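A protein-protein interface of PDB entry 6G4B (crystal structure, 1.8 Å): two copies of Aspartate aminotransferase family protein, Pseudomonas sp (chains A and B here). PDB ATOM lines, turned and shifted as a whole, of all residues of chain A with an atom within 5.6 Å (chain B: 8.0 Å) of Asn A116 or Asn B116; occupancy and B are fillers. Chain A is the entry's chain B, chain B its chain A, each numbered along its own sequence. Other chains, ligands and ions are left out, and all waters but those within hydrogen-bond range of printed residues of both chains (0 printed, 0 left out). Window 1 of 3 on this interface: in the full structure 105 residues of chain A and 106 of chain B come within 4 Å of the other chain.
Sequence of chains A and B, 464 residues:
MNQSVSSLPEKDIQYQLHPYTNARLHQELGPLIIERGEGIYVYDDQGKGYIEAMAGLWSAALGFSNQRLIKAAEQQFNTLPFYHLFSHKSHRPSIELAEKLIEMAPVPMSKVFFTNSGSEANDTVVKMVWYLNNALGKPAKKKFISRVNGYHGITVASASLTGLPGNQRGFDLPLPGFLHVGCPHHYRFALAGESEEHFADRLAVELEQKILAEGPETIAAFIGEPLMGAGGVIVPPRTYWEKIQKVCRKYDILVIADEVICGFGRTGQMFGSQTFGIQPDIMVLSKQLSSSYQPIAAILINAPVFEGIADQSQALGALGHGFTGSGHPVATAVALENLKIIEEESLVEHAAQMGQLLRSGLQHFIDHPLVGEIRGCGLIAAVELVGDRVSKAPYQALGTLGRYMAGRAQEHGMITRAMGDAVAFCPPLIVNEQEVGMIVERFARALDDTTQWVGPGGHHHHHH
Asn A116 touches its own counterpart, Asn B116.
Asn A116 touches Ser B117, and with the chains exchanged Ser A117 touches Asn B116.
Ser A117 touches Glu B120, and with the chains exchanged Glu A120 touches Ser B117.
Pro B295 touches its own counterpart, Pro A295.
OG of Ser B117 is in hydrogen-bond range of OE2 of Glu A120 (2.5 Å).
The side-chain carboxylate (OE2) of Glu B120 is in hydrogen-bond range of the side-chain hydroxyl (OG) of Ser A117, at 2.5 Å.
The side-chain carboxylate (OE2) of Glu A120 lies close to the side-chain carboxylate (OE2) of Glu B120 (3.5 Å).
Asn A116 touches just these residues of chain B: Asn B116, Ser B117 and Pro B295.
Of the printed residues of chain B, Pro A295 touches Asn B116 and Pro B295.
Printed residues of chain A within 4 Å of Ser B117: Asn A116 and Glu A120.
Of the printed residues of chain A, Glu B120 touches Ser A117 (2.5 Å) and Glu A120 (3.4 Å).
Ala B298 touches none of the printed residues of chain A.
His B328 touches none of the printed residues of chain A.
The nearest residue of chain B that does not touch Asn A116 is Glu B120 (4.8 Å).
The nearest residue of chain A that does not touch Asn B116 is Glu A120 (4.7 Å).
The nearest printed residue of chain A that does not touch Pro B295 is His A328 (4.5 Å).
Among the printed residues, merely in contact across the chains: Asn A116 with Asn B116 (3.7 Å), Asn A116 with Ser B117 (3.7 Å), Asn A116 with Pro B295 (3.4 Å), Ser A117 with Asn B116 (3.6 Å), Pro A295 with Asn B116 (3.5 Å), Pro A295 with Pro B295 (3.99 Å) and Phe A323 with Ser B119 (3.8 Å).
The backbone NH (N) of Asn B116 is in hydrogen-bond range of the side-chain carboxylate (OE1) of Glu B120 (2.6 Å).
N of Ile B296 is in hydrogen-bond range of O of Asn B116 (3.1 Å).
The backbone NH (N) of Glu B120 is in hydrogen-bond range of the side-chain hydroxyl (OG) of Ser B117 (2.9 Å).
OG1 of Thr B124 lies within hydrogen-bond range of O of Glu B120, 2.8 Å away.
The side-chain hydroxyl (OG) of Ser A117 is in hydrogen-bond range of the backbone NH (N) of Glu A120 (3.0 Å).
N of Phe A323 is in hydrogen-bond range of OG of Ser A326, at 3.1 Å.
Of the 28 printed residues of chain B, 5 touch a printed residue of chain A.
Among the printed residues, 10 pairs touch across the chains.
Among the printed residues, no Asp or Glu carboxylate lies within 4 Å of a Lys or Arg side-chain nitrogen of the other chain.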
ATOM      1  N   PHE A 114      14.526  -8.884   9.632  1.00  0.00           N
ATOM      2  CA  PHE A 114      14.570  -7.791  10.587  1.00  0.00           C
ATOM      3  C   PHE A 114      15.745  -7.927  11.554  1.00  0.00           C
ATOM      4  O   PHE A 114      16.107  -9.021  11.985  1.00  0.00           O
ATOM      5  CB  PHE A 114      13.272  -7.699  11.410  1.00  0.00           C
ATOM      6  CG  PHE A 114      12.054  -7.258  10.624  1.00  0.00           C
ATOM      7  CD1 PHE A 114      11.954  -5.966  10.157  1.00  0.00           C
ATOM      8  CD2 PHE A 114      11.018  -8.137  10.364  1.00  0.00           C
ATOM      9  CE1 PHE A 114      10.839  -5.542   9.464  1.00  0.00           C
ATOM     10  CE2 PHE A 114       9.891  -7.730   9.655  1.00  0.00           C
ATOM     11  CZ  PHE A 114       9.797  -6.419   9.217  1.00  0.00           C
ATOM     12  N   THR A 115      16.293  -6.771  11.941  1.00  0.00           N
ATOM     13  CA  THR A 115      17.284  -6.676  13.004  1.00  0.00           C
ATOM     14  C   THR A 115      16.941  -5.492  13.907  1.00  0.00           C
ATOM     15  O   THR A 115      15.958  -4.777  13.675  1.00  0.00           O
ATOM     16  CB  THR A 115      18.712  -6.485  12.453  1.00  0.00           C
ATOM     17  OG1 THR A 115      18.831  -5.180  11.842  1.00  0.00           O
ATOM     18  CG2 THR A 115      19.052  -7.554  11.413  1.00  0.00           C
ATOM     19  N   ASN A 116      17.769  -5.252  14.920  1.00  0.00           N
ATOM     20  CA  ASN A 116      17.560  -4.080  15.793  1.00  0.00           C
ATOM     21  C   ASN A 116      18.204  -2.814  15.232  1.00  0.00           C
ATOM     22  O   ASN A 116      17.684  -1.719  15.426  1.00  0.00           O
ATOM     23  CB  ASN A 116      18.112  -4.310  17.187  1.00  0.00           C
ATOM     24  CG  ASN A 116      17.587  -5.583  17.835  1.00  0.00           C
ATOM     25  OD1 ASN A 116      16.401  -5.716  18.105  1.00  0.00           O
ATOM     26  ND2 ASN A 116      18.474  -6.542  18.037  1.00  0.00           N
ATOM     27  N   SER A 117      19.369  -2.946  14.610  1.00  0.00           N
ATOM     28  CA  SER A 117      20.164  -1.789  14.174  1.00  0.00           C
ATOM     29  C   SER A 117      20.664  -1.894  12.735  1.00  0.00           C
ATOM     30  O   SER A 117      20.767  -2.990  12.182  1.00  0.00           O
ATOM     31  CB  SER A 117      21.392  -1.604  15.062  1.00  0.00           C
ATOM     32  OG  SER A 117      22.316  -2.666  14.908  1.00  0.00           O
ATOM     33  N   GLY A 118      21.022  -0.731  12.178  1.00  0.00           N
ATOM     34  CA  GLY A 118      21.673  -0.693  10.870  1.00  0.00           C
ATOM     35  C   GLY A 118      22.994  -1.446  10.870  1.00  0.00           C
ATOM     36  O   GLY A 118      23.324  -2.117   9.901  1.00  0.00           O
ATOM     37  N   GLU A 120      23.833  -4.066  12.790  1.00  0.00           N
ATOM     38  CA  GLU A 120      23.481  -5.479  12.747  1.00  0.00           C
ATOM     39  C   GLU A 120      22.986  -5.875  11.350  1.00  0.00           C
ATOM     40  O   GLU A 120      23.261  -6.981  10.876  1.00  0.00           O
ATOM     41  CB  GLU A 120      22.354  -5.805  13.718  1.00  0.00           C
ATOM     42  CG  GLU A 120      22.683  -5.888  15.204  1.00  0.00           C
ATOM     43  CD  GLU A 120      21.388  -6.004  16.020  1.00  0.00           C
ATOM     44  OE1 GLU A 120      20.313  -5.703  15.434  1.00  0.00           O
ATOM     45  OE2 GLU A 120      21.430  -6.357  17.224  1.00  0.00           O
ATOM     46  N   SER A 286      16.641   1.597   8.182  1.00  0.00           N
ATOM     47  CA  SER A 286      16.647   1.786   9.636  1.00  0.00           C
ATOM     48  C   SER A 286      16.104   3.186   9.929  1.00  0.00           C
ATOM     49  O   SER A 286      15.400   3.737   9.095  1.00  0.00           O
ATOM     50  CB  SER A 286      18.068   1.620  10.179  1.00  0.00           C
ATOM     51  OG  SER A 286      18.051   1.556  11.588  1.00  0.00           O
ATOM     52  N   PRO A 295      14.211   0.685  18.388  1.00  0.00           N
ATOM     53  CA  PRO A 295      15.334   0.158  17.603  1.00  0.00           C
ATOM     54  C   PRO A 295      14.824  -0.912  16.646  1.00  0.00           C
ATOM     55  O   PRO A 295      14.431  -1.994  17.083  1.00  0.00           O
ATOM     56  CB  PRO A 295      16.274  -0.442  18.646  1.00  0.00           C
ATOM     57  CG  PRO A 295      15.711  -0.105  19.988  1.00  0.00           C
ATOM     58  CD  PRO A 295      14.246   0.209  19.782  1.00  0.00           C
ATOM     59  N   ILE A 296      14.806  -0.599  15.361  1.00  0.00           N
ATOM     60  CA  ILE A 296      14.461  -1.585  14.357  1.00  0.00           C
ATOM     61  C   ILE A 296      15.146  -1.225  13.040  1.00  0.00           C
ATOM     62  O   ILE A 296      15.193  -0.056  12.634  1.00  0.00           O
ATOM     63  CB  ILE A 296      12.927  -1.746  14.176  1.00  0.00           C
ATOM     64  CG1 ILE A 296      12.600  -2.686  13.018  1.00  0.00           C
ATOM     65  CG2 ILE A 296      12.235  -0.397  13.950  1.00  0.00           C
ATOM     66  CD1 ILE A 296      11.141  -3.089  12.979  1.00  0.00           C
ATOM     67  N   ALA A 297      15.678  -2.249  12.385  1.00  0.00           N
ATOM     68  CA  ALA A 297      16.191  -2.142  11.012  1.00  0.00           C
ATOM     69  C   ALA A 297      15.647  -3.321  10.192  1.00  0.00           C
ATOM     70  O   ALA A 297      15.168  -4.318  10.751  1.00  0.00           O
ATOM     71  CB  ALA A 297      17.694  -2.138  11.019  1.00  0.00           C
ATOM     72  N   PHE A 323      18.472 -12.440  15.581  1.00  0.00           N
ATOM     73  CA  PHE A 323      18.581 -11.721  16.839  1.00  0.00           C
ATOM     74  C   PHE A 323      17.307 -11.967  17.633  1.00  0.00           C
ATOM     75  O   PHE A 323      16.215 -12.105  17.078  1.00  0.00           O
ATOM     76  CB  PHE A 323      18.755 -10.215  16.587  1.00  0.00           C
ATOM     77  CG  PHE A 323      19.972  -9.891  15.763  1.00  0.00           C
ATOM     78  CD1 PHE A 323      21.213  -9.725  16.366  1.00  0.00           C
ATOM     79  CD2 PHE A 323      19.881  -9.779  14.382  1.00  0.00           C
ATOM     80  CE1 PHE A 323      22.357  -9.470  15.591  1.00  0.00           C
ATOM     81  CE2 PHE A 323      21.015  -9.531  13.609  1.00  0.00           C
ATOM     82  CZ  PHE A 323      22.249  -9.375  14.215  1.00  0.00           C
ATOM     83  N   GLY A 325      15.636  -9.867  19.200  1.00  0.00           N
ATOM     84  CA  GLY A 325      14.790  -8.749  18.862  1.00  0.00           C
ATOM     85  C   GLY A 325      14.383  -8.648  17.405  1.00  0.00           C
ATOM     86  O   GLY A 325      13.674  -7.723  17.047  1.00  0.00           O
ATOM     87  N   SER A 326      14.816  -9.583  16.555  1.00  0.00           N
ATOM     88  CA  SER A 326      14.431  -9.555  15.143  1.00  0.00           C
ATOM     89  C   SER A 326      12.924  -9.543  15.009  1.00  0.00           C
ATOM     90  O   SER A 326      12.253 -10.518  15.311  1.00  0.00           O
ATOM     91  CB  SER A 326      14.987 -10.761  14.366  1.00  0.00           C
ATOM     92  OG  SER A 326      16.397 -10.631  14.136  1.00  0.00           O
ATOM     93  N   HIS A 328      10.816  -7.576  16.553  1.00  0.00           N
ATOM     94  CA  HIS A 328      10.151  -7.311  17.830  1.00  0.00           C
ATOM     95  C   HIS A 328       8.750  -6.689  17.617  1.00  0.00           C
ATOM     96  O   HIS A 328       8.610  -5.715  16.889  1.00  0.00           O
ATOM     97  CB  HIS A 328      10.986  -6.364  18.672  1.00  0.00           C
ATOM     98  CG  HIS A 328      10.552  -6.286  20.108  1.00  0.00           C
ATOM     99  ND1 HIS A 328       9.439  -5.584  20.516  1.00  0.00           N
ATOM    100  CD2 HIS A 328      11.098  -6.802  21.229  1.00  0.00           C
ATOM    101  CE1 HIS A 328       9.310  -5.685  21.824  1.00  0.00           C
ATOM    102  NE2 HIS A 328      10.312  -6.408  22.282  1.00  0.00           N
ATOM    103  N   PHE B 113      28.267   0.583  29.032  1.00  0.00           N
ATOM    104  CA  PHE B 113      28.094   0.939  27.631  1.00  0.00           C
ATOM    105  C   PHE B 113      26.871   0.161  27.138  1.00  0.00           C
ATOM    106  O   PHE B 113      26.777  -1.050  27.352  1.00  0.00           O
ATOM    107  CB  PHE B 113      29.328   0.578  26.799  1.00  0.00           C
ATOM    108  CG  PHE B 113      29.305   1.176  25.418  1.00  0.00           C
ATOM    109  CD1 PHE B 113      28.655   0.526  24.355  1.00  0.00           C
ATOM    110  CD2 PHE B 113      29.914   2.410  25.177  1.00  0.00           C
ATOM    111  CE1 PHE B 113      28.610   1.107  23.085  1.00  0.00           C
ATOM    112  CE2 PHE B 113      29.860   2.988  23.917  1.00  0.00           C
ATOM    113  CZ  PHE B 113      29.230   2.329  22.871  1.00  0.00           C
ATOM    114  N   PHE B 114      25.948   0.863  26.509  1.00  0.00           N
ATOM    115  CA  PHE B 114      24.685   0.252  26.084  1.00  0.00           C
ATOM    116  C   PHE B 114      24.689  -0.086  24.605  1.00  0.00           C
ATOM    117  O   PHE B 114      25.248   0.655  23.772  1.00  0.00           O
ATOM    118  CB  PHE B 114      23.494   1.188  26.358  1.00  0.00           C
ATOM    119  CG  PHE B 114      23.171   1.376  27.824  1.00  0.00           C
ATOM    120  CD1 PHE B 114      22.661   0.325  28.565  1.00  0.00           C
ATOM    121  CD2 PHE B 114      23.350   2.602  28.440  1.00  0.00           C
ATOM    122  CE1 PHE B 114      22.331   0.478  29.896  1.00  0.00           C
ATOM    123  CE2 PHE B 114      23.039   2.769  29.784  1.00  0.00           C
ATOM    124  CZ  PHE B 114      22.512   1.710  30.515  1.00  0.00           C
ATOM    125  N   THR B 115      24.025  -1.193  24.285  1.00  0.00           N
ATOM    126  CA  THR B 115      23.752  -1.585  22.905  1.00  0.00           C
ATOM    127  C   THR B 115      22.303  -2.063  22.806  1.00  0.00           C
ATOM    128  O   THR B 115      21.555  -2.057  23.799  1.00  0.00           O
ATOM    129  CB  THR B 115      24.693  -2.735  22.441  1.00  0.00           C
ATOM    130  OG1 THR B 115      24.365  -3.942  23.140  1.00  0.00           O
ATOM    131  CG2 THR B 115      26.159  -2.389  22.689  1.00  0.00           C
ATOM    132  N   ASN B 116      21.891  -2.488  21.613  1.00  0.00           N
ATOM    133  CA  ASN B 116      20.537  -3.044  21.439  1.00  0.00           C
ATOM    134  C   ASN B 116      20.452  -4.518  21.742  1.00  0.00           C
ATOM    135  O   ASN B 116      19.416  -4.973  22.209  1.00  0.00           O
ATOM    136  CB  ASN B 116      20.002  -2.831  20.021  1.00  0.00           C
ATOM    137  CG  ASN B 116      20.073  -1.379  19.588  1.00  0.00           C
ATOM    138  OD1 ASN B 116      19.390  -0.503  20.137  1.00  0.00           O
ATOM    139  ND2 ASN B 116      20.935  -1.109  18.625  1.00  0.00           N
ATOM    140  N   SER B 117      21.502  -5.266  21.420  1.00  0.00           N
ATOM    141  CA  SER B 117      21.472  -6.716  21.530  1.00  0.00           C
ATOM    142  C   SER B 117      22.715  -7.296  22.197  1.00  0.00           C
ATOM    143  O   SER B 117      23.770  -6.674  22.222  1.00  0.00           O
ATOM    144  CB  SER B 117      21.358  -7.344  20.130  1.00  0.00           C
ATOM    145  OG  SER B 117      22.538  -7.131  19.372  1.00  0.00           O
ATOM    146  N   GLY B 118      22.575  -8.532  22.663  1.00  0.00           N
ATOM    147  CA  GLY B 118      23.702  -9.295  23.197  1.00  0.00           C
ATOM    148  C   GLY B 118      24.771  -9.515  22.143  1.00  0.00           C
ATOM    149  O   GLY B 118      25.969  -9.456  22.454  1.00  0.00           O
ATOM    150  N   SER B 119      24.362  -9.756  20.899  1.00  0.00           N
ATOM    151  CA  SER B 119      25.331  -9.936  19.822  1.00  0.00           C
ATOM    152  C   SER B 119      26.128  -8.673  19.588  1.00  0.00           C
ATOM    153  O   SER B 119      27.355  -8.733  19.479  1.00  0.00           O
ATOM    154  CB  SER B 119      24.654 -10.312  18.503  1.00  0.00           C
ATOM    155  OG  SER B 119      23.948 -11.527  18.594  1.00  0.00           O
ATOM    156  N   GLU B 120      25.448  -7.524  19.521  1.00  0.00           N
ATOM    157  CA  GLU B 120      26.161  -6.231  19.441  1.00  0.00           C
ATOM    158  C   GLU B 120      27.063  -5.991  20.644  1.00  0.00           C
ATOM    159  O   GLU B 120      28.167  -5.454  20.510  1.00  0.00           O
ATOM    160  CB  GLU B 120      25.191  -5.060  19.375  1.00  0.00           C
ATOM    161  CG  GLU B 120      24.429  -4.817  18.072  1.00  0.00           C
ATOM    162  CD  GLU B 120      23.338  -3.755  18.280  1.00  0.00           C
ATOM    163  OE1 GLU B 120      23.039  -3.471  19.461  1.00  0.00           O
ATOM    164  OE2 GLU B 120      22.799  -3.189  17.303  1.00  0.00           O
ATOM    165  N   ALA B 121      26.607  -6.385  21.820  1.00  0.00           N
ATOM    166  CA  ALA B 121      27.393  -6.161  23.036  1.00  0.00           C
ATOM    167  C   ALA B 121      28.702  -6.968  22.998  1.00  0.00           C
ATOM    168  O   ALA B 121      29.774  -6.422  23.259  1.00  0.00           O
ATOM    169  CB  ALA B 121      26.568  -6.502  24.271  1.00  0.00           C
ATOM    170  N   THR B 124      30.993  -5.532  20.436  1.00  0.00           N
ATOM    171  CA  THR B 124      31.597  -4.344  21.025  1.00  0.00           C
ATOM    172  C   THR B 124      32.728  -4.690  21.996  1.00  0.00           C
ATOM    173  O   THR B 124      33.785  -4.053  22.007  1.00  0.00           O
ATOM    174  CB  THR B 124      30.518  -3.500  21.721  1.00  0.00           C
ATOM    175  OG1 THR B 124      29.594  -3.024  20.724  1.00  0.00           O
ATOM    176  CG2 THR B 124      31.123  -2.308  22.428  1.00  0.00           C
ATOM    177  N   LEU B 285      25.176  -8.165  29.545  1.00  0.00           N
ATOM    178  CA  LEU B 285      23.808  -8.347  29.989  1.00  0.00           C
ATOM    179  C   LEU B 285      22.817  -8.065  28.878  1.00  0.00           C
ATOM    180  O   LEU B 285      23.043  -7.190  28.026  1.00  0.00           O
ATOM    181  CB  LEU B 285      23.517  -7.389  31.137  1.00  0.00           C
ATOM    182  CG  LEU B 285      24.446  -7.539  32.341  1.00  0.00           C
ATOM    183  CD1 LEU B 285      24.375  -6.297  33.213  1.00  0.00           C
ATOM    184  CD2 LEU B 285      24.067  -8.779  33.123  1.00  0.00           C
ATOM    185  N   SER B 286      21.705  -8.780  28.895  1.00  0.00           N
ATOM    186  CA  SER B 286      20.646  -8.544  27.911  1.00  0.00           C
ATOM    187  C   SER B 286      19.361  -9.188  28.430  1.00  0.00           C
ATOM    188  O   SER B 286      19.231  -9.420  29.633  1.00  0.00           O
ATOM    189  CB  SER B 286      21.056  -9.107  26.550  1.00  0.00           C
ATOM    190  OG  SER B 286      20.159  -8.679  25.549  1.00  0.00           O
ATOM    191  N   LYS B 287      18.413  -9.454  27.536  1.00  0.00           N
ATOM    192  CA  LYS B 287      17.274 -10.367  27.806  1.00  0.00           C
ATOM    193  C   LYS B 287      16.462  -9.955  29.040  1.00  0.00           C
ATOM    194  O   LYS B 287      15.633  -9.051  28.946  1.00  0.00           O
ATOM    195  CB  LYS B 287      17.740 -11.819  27.881  1.00  0.00           C
ATOM    196  CG  LYS B 287      18.154 -12.391  26.521  1.00  0.00           C
ATOM    197  CD  LYS B 287      18.408 -13.905  26.615  1.00  0.00           C
ATOM    198  CE  LYS B 287      18.843 -14.529  25.284  1.00  0.00           C
ATOM    199  NZ  LYS B 287      17.875 -14.324  24.168  1.00  0.00           N
ATOM    200  N   LEU B 289      17.174  -8.206  31.390  1.00  0.00           N
ATOM    201  CA  LEU B 289      17.379  -6.778  31.679  1.00  0.00           C
ATOM    202  C   LEU B 289      16.093  -5.976  31.504  1.00  0.00           C
ATOM    203  O   LEU B 289      15.796  -5.123  32.327  1.00  0.00           O
ATOM    204  CB  LEU B 289      18.476  -6.222  30.763  1.00  0.00           C
ATOM    205  CG  LEU B 289      18.833  -4.740  30.844  1.00  0.00           C
ATOM    206  CD1 LEU B 289      19.170  -4.311  32.261  1.00  0.00           C
ATOM    207  CD2 LEU B 289      20.003  -4.499  29.919  1.00  0.00           C
ATOM    208  N   SER B 290      15.345  -6.236  30.429  1.00  0.00           N
ATOM    209  CA  SER B 290      14.079  -5.526  30.158  1.00  0.00           C
ATOM    210  C   SER B 290      12.897  -6.469  30.026  1.00  0.00           C
ATOM    211  O   SER B 290      11.846  -6.070  29.534  1.00  0.00           O
ATOM    212  CB  SER B 290      14.184  -4.700  28.866  1.00  0.00           C
ATOM    213  OG  SER B 290      14.332  -5.577  27.761  1.00  0.00           O
ATOM    214  N   GLN B 294      11.822  -4.423  25.466  1.00  0.00           N
ATOM    215  CA  GLN B 294      12.551  -3.561  24.546  1.00  0.00           C
ATOM    216  C   GLN B 294      13.903  -4.197  24.219  1.00  0.00           C
ATOM    217  O   GLN B 294      14.493  -4.877  25.056  1.00  0.00           O
ATOM    218  CB  GLN B 294      12.810  -2.202  25.209  1.00  0.00           C
ATOM    219  CG  GLN B 294      11.559  -1.415  25.458  1.00  0.00           C
ATOM    220  CD  GLN B 294      11.051  -0.785  24.188  1.00  0.00           C
ATOM    221  OE1 GLN B 294      11.504   0.288  23.800  1.00  0.00           O
ATOM    222  NE2 GLN B 294      10.136  -1.459  23.518  1.00  0.00           N
ATOM    223  N   PRO B 295      14.429  -3.957  23.009  1.00  0.00           N
ATOM    224  CA  PRO B 295      15.781  -4.451  22.702  1.00  0.00           C
ATOM    225  C   PRO B 295      16.810  -3.582  23.420  1.00  0.00           C
ATOM    226  O   PRO B 295      16.970  -2.410  23.092  1.00  0.00           O
ATOM    227  CB  PRO B 295      15.894  -4.290  21.178  1.00  0.00           C
ATOM    228  CG  PRO B 295      14.551  -3.855  20.697  1.00  0.00           C
ATOM    229  CD  PRO B 295      13.806  -3.286  21.860  1.00  0.00           C
ATOM    230  N   ILE B 296      17.461  -4.141  24.441  1.00  0.00           N
ATOM    231  CA  ILE B 296      18.534  -3.435  25.126  1.00  0.00           C
ATOM    232  C   ILE B 296      19.500  -4.455  25.718  1.00  0.00           C
ATOM    233  O   ILE B 296      19.080  -5.494  26.250  1.00  0.00           O
ATOM    234  CB  ILE B 296      18.013  -2.447  26.196  1.00  0.00           C
ATOM    235  CG1 ILE B 296      19.166  -1.831  26.973  1.00  0.00           C
ATOM    236  CG2 ILE B 296      17.031  -3.121  27.158  1.00  0.00           C
ATOM    237  CD1 ILE B 296      18.733  -0.657  27.832  1.00  0.00           C
ATOM    238  N   ALA B 297      20.785  -4.146  25.589  1.00  0.00           N
ATOM    239  CA  ALA B 297      21.832  -4.888  26.242  1.00  0.00           C
ATOM    240  C   ALA B 297      22.815  -3.897  26.856  1.00  0.00           C
ATOM    241  O   ALA B 297      22.812  -2.706  26.508  1.00  0.00           O
ATOM    242  CB  ALA B 297      22.533  -5.810  25.234  1.00  0.00           C
ATOM    243  N   ALA B 298      23.675  -4.405  27.734  1.00  0.00           N
ATOM    244  CA  ALA B 298      24.608  -3.560  28.464  1.00  0.00           C
ATOM    245  C   ALA B 298      25.918  -4.279  28.682  1.00  0.00           C
ATOM    246  O   ALA B 298      25.938  -5.489  28.932  1.00  0.00           O
ATOM    247  CB  ALA B 298      23.999  -3.142  29.788  1.00  0.00           C
ATOM    248  N   GLY B 322      29.504   3.345  18.478  1.00  0.00           N
ATOM    249  CA  GLY B 322      28.204   3.563  19.100  1.00  0.00           C
ATOM    250  C   GLY B 322      27.068   3.241  18.159  1.00  0.00           C
ATOM    251  O   GLY B 322      27.201   3.445  16.941  1.00  0.00           O
ATOM    252  N   PHE B 323      25.962   2.757  18.727  1.00  0.00           N
ATOM    253  CA  PHE B 323      24.745   2.465  17.977  1.00  0.00           C
ATOM    254  C   PHE B 323      23.751   3.607  18.161  1.00  0.00           C
ATOM    255  O   PHE B 323      23.696   4.221  19.233  1.00  0.00           O
ATOM    256  CB  PHE B 323      24.137   1.145  18.453  1.00  0.00           C
ATOM    257  CG  PHE B 323      25.088  -0.026  18.344  1.00  0.00           C
ATOM    258  CD1 PHE B 323      25.206  -0.732  17.156  1.00  0.00           C
ATOM    259  CD2 PHE B 323      25.895  -0.389  19.413  1.00  0.00           C
ATOM    260  CE1 PHE B 323      26.112  -1.771  17.038  1.00  0.00           C
ATOM    261  CE2 PHE B 323      26.800  -1.461  19.312  1.00  0.00           C
ATOM    262  CZ  PHE B 323      26.902  -2.147  18.122  1.00  0.00           C
ATOM    263  N   THR B 324      22.959   3.888  17.134  1.00  0.00           N
ATOM    264  CA  THR B 324      21.935   4.900  17.270  1.00  0.00           C
ATOM    265  C   THR B 324      21.079   4.659  18.516  1.00  0.00           C
ATOM    266  O   THR B 324      20.769   5.593  19.277  1.00  0.00           O
ATOM    267  CB  THR B 324      21.081   4.953  16.004  1.00  0.00           C
ATOM    268  OG1 THR B 324      21.870   5.507  14.936  1.00  0.00           O
ATOM    269  CG2 THR B 324      19.833   5.810  16.225  1.00  0.00           C
ATOM    270  N   GLY B 325      20.733   3.390  18.719  1.00  0.00           N
ATOM    271  CA  GLY B 325      19.904   2.961  19.813  1.00  0.00           C
ATOM    272  C   GLY B 325      20.623   2.763  21.134  1.00  0.00           C
ATOM    273  O   GLY B 325      19.975   2.383  22.108  1.00  0.00           O
ATOM    274  N   SER B 326      21.941   2.987  21.187  1.00  0.00           N
ATOM    275  CA  SER B 326      22.676   2.835  22.452  1.00  0.00           C
ATOM    276  C   SER B 326      22.047   3.701  23.539  1.00  0.00           C
ATOM    277  O   SER B 326      22.079   4.942  23.465  1.00  0.00           O
ATOM    278  CB  SER B 326      24.151   3.229  22.305  1.00  0.00           C
ATOM    279  OG  SER B 326      24.881   2.244  21.591  1.00  0.00           O
ATOM    280  N   GLY B 327      21.470   3.034  24.528  1.00  0.00           N
ATOM    281  CA  GLY B 327      20.893   3.708  25.671  1.00  0.00           C
ATOM    282  C   GLY B 327      19.531   4.326  25.395  1.00  0.00           C
ATOM    283  O   GLY B 327      19.103   5.201  26.144  1.00  0.00           O
ATOM    284  N   HIS B 328      18.852   3.876  24.334  1.00  0.00           N
ATOM    285  CA  HIS B 328      17.572   4.453  23.915  1.00  0.00           C
ATOM    286  C   HIS B 328      16.703   4.761  25.126  1.00  0.00           C
ATOM    287  O   HIS B 328      16.529   3.899  25.990  1.00  0.00           O
ATOM    288  CB  HIS B 328      16.851   3.451  23.008  1.00  0.00           C
ATOM    289  CG  HIS B 328      15.667   4.017  22.305  1.00  0.00           C
ATOM    290  ND1 HIS B 328      14.464   4.252  22.937  1.00  0.00           N
ATOM    291  CD2 HIS B 328      15.491   4.374  21.011  1.00  0.00           C
ATOM    292  CE1 HIS B 328      13.604   4.757  22.067  1.00  0.00           C
ATOM    293  NE2 HIS B 328      14.199   4.829  20.890  1.00  0.00           N
ATOM    294  N   ALA B 331      13.896   2.181  25.935  1.00  0.00           N
ATOM    295  CA  ALA B 331      14.451   0.891  26.316  1.00  0.00           C
ATOM    296  C   ALA B 331      15.095   0.947  27.701  1.00  0.00           C
ATOM    297  O   ALA B 331      14.894   0.043  28.516  1.00  0.00           O
ATOM    298  CB  ALA B 331      15.435   0.422  25.275  1.00  0.00           C
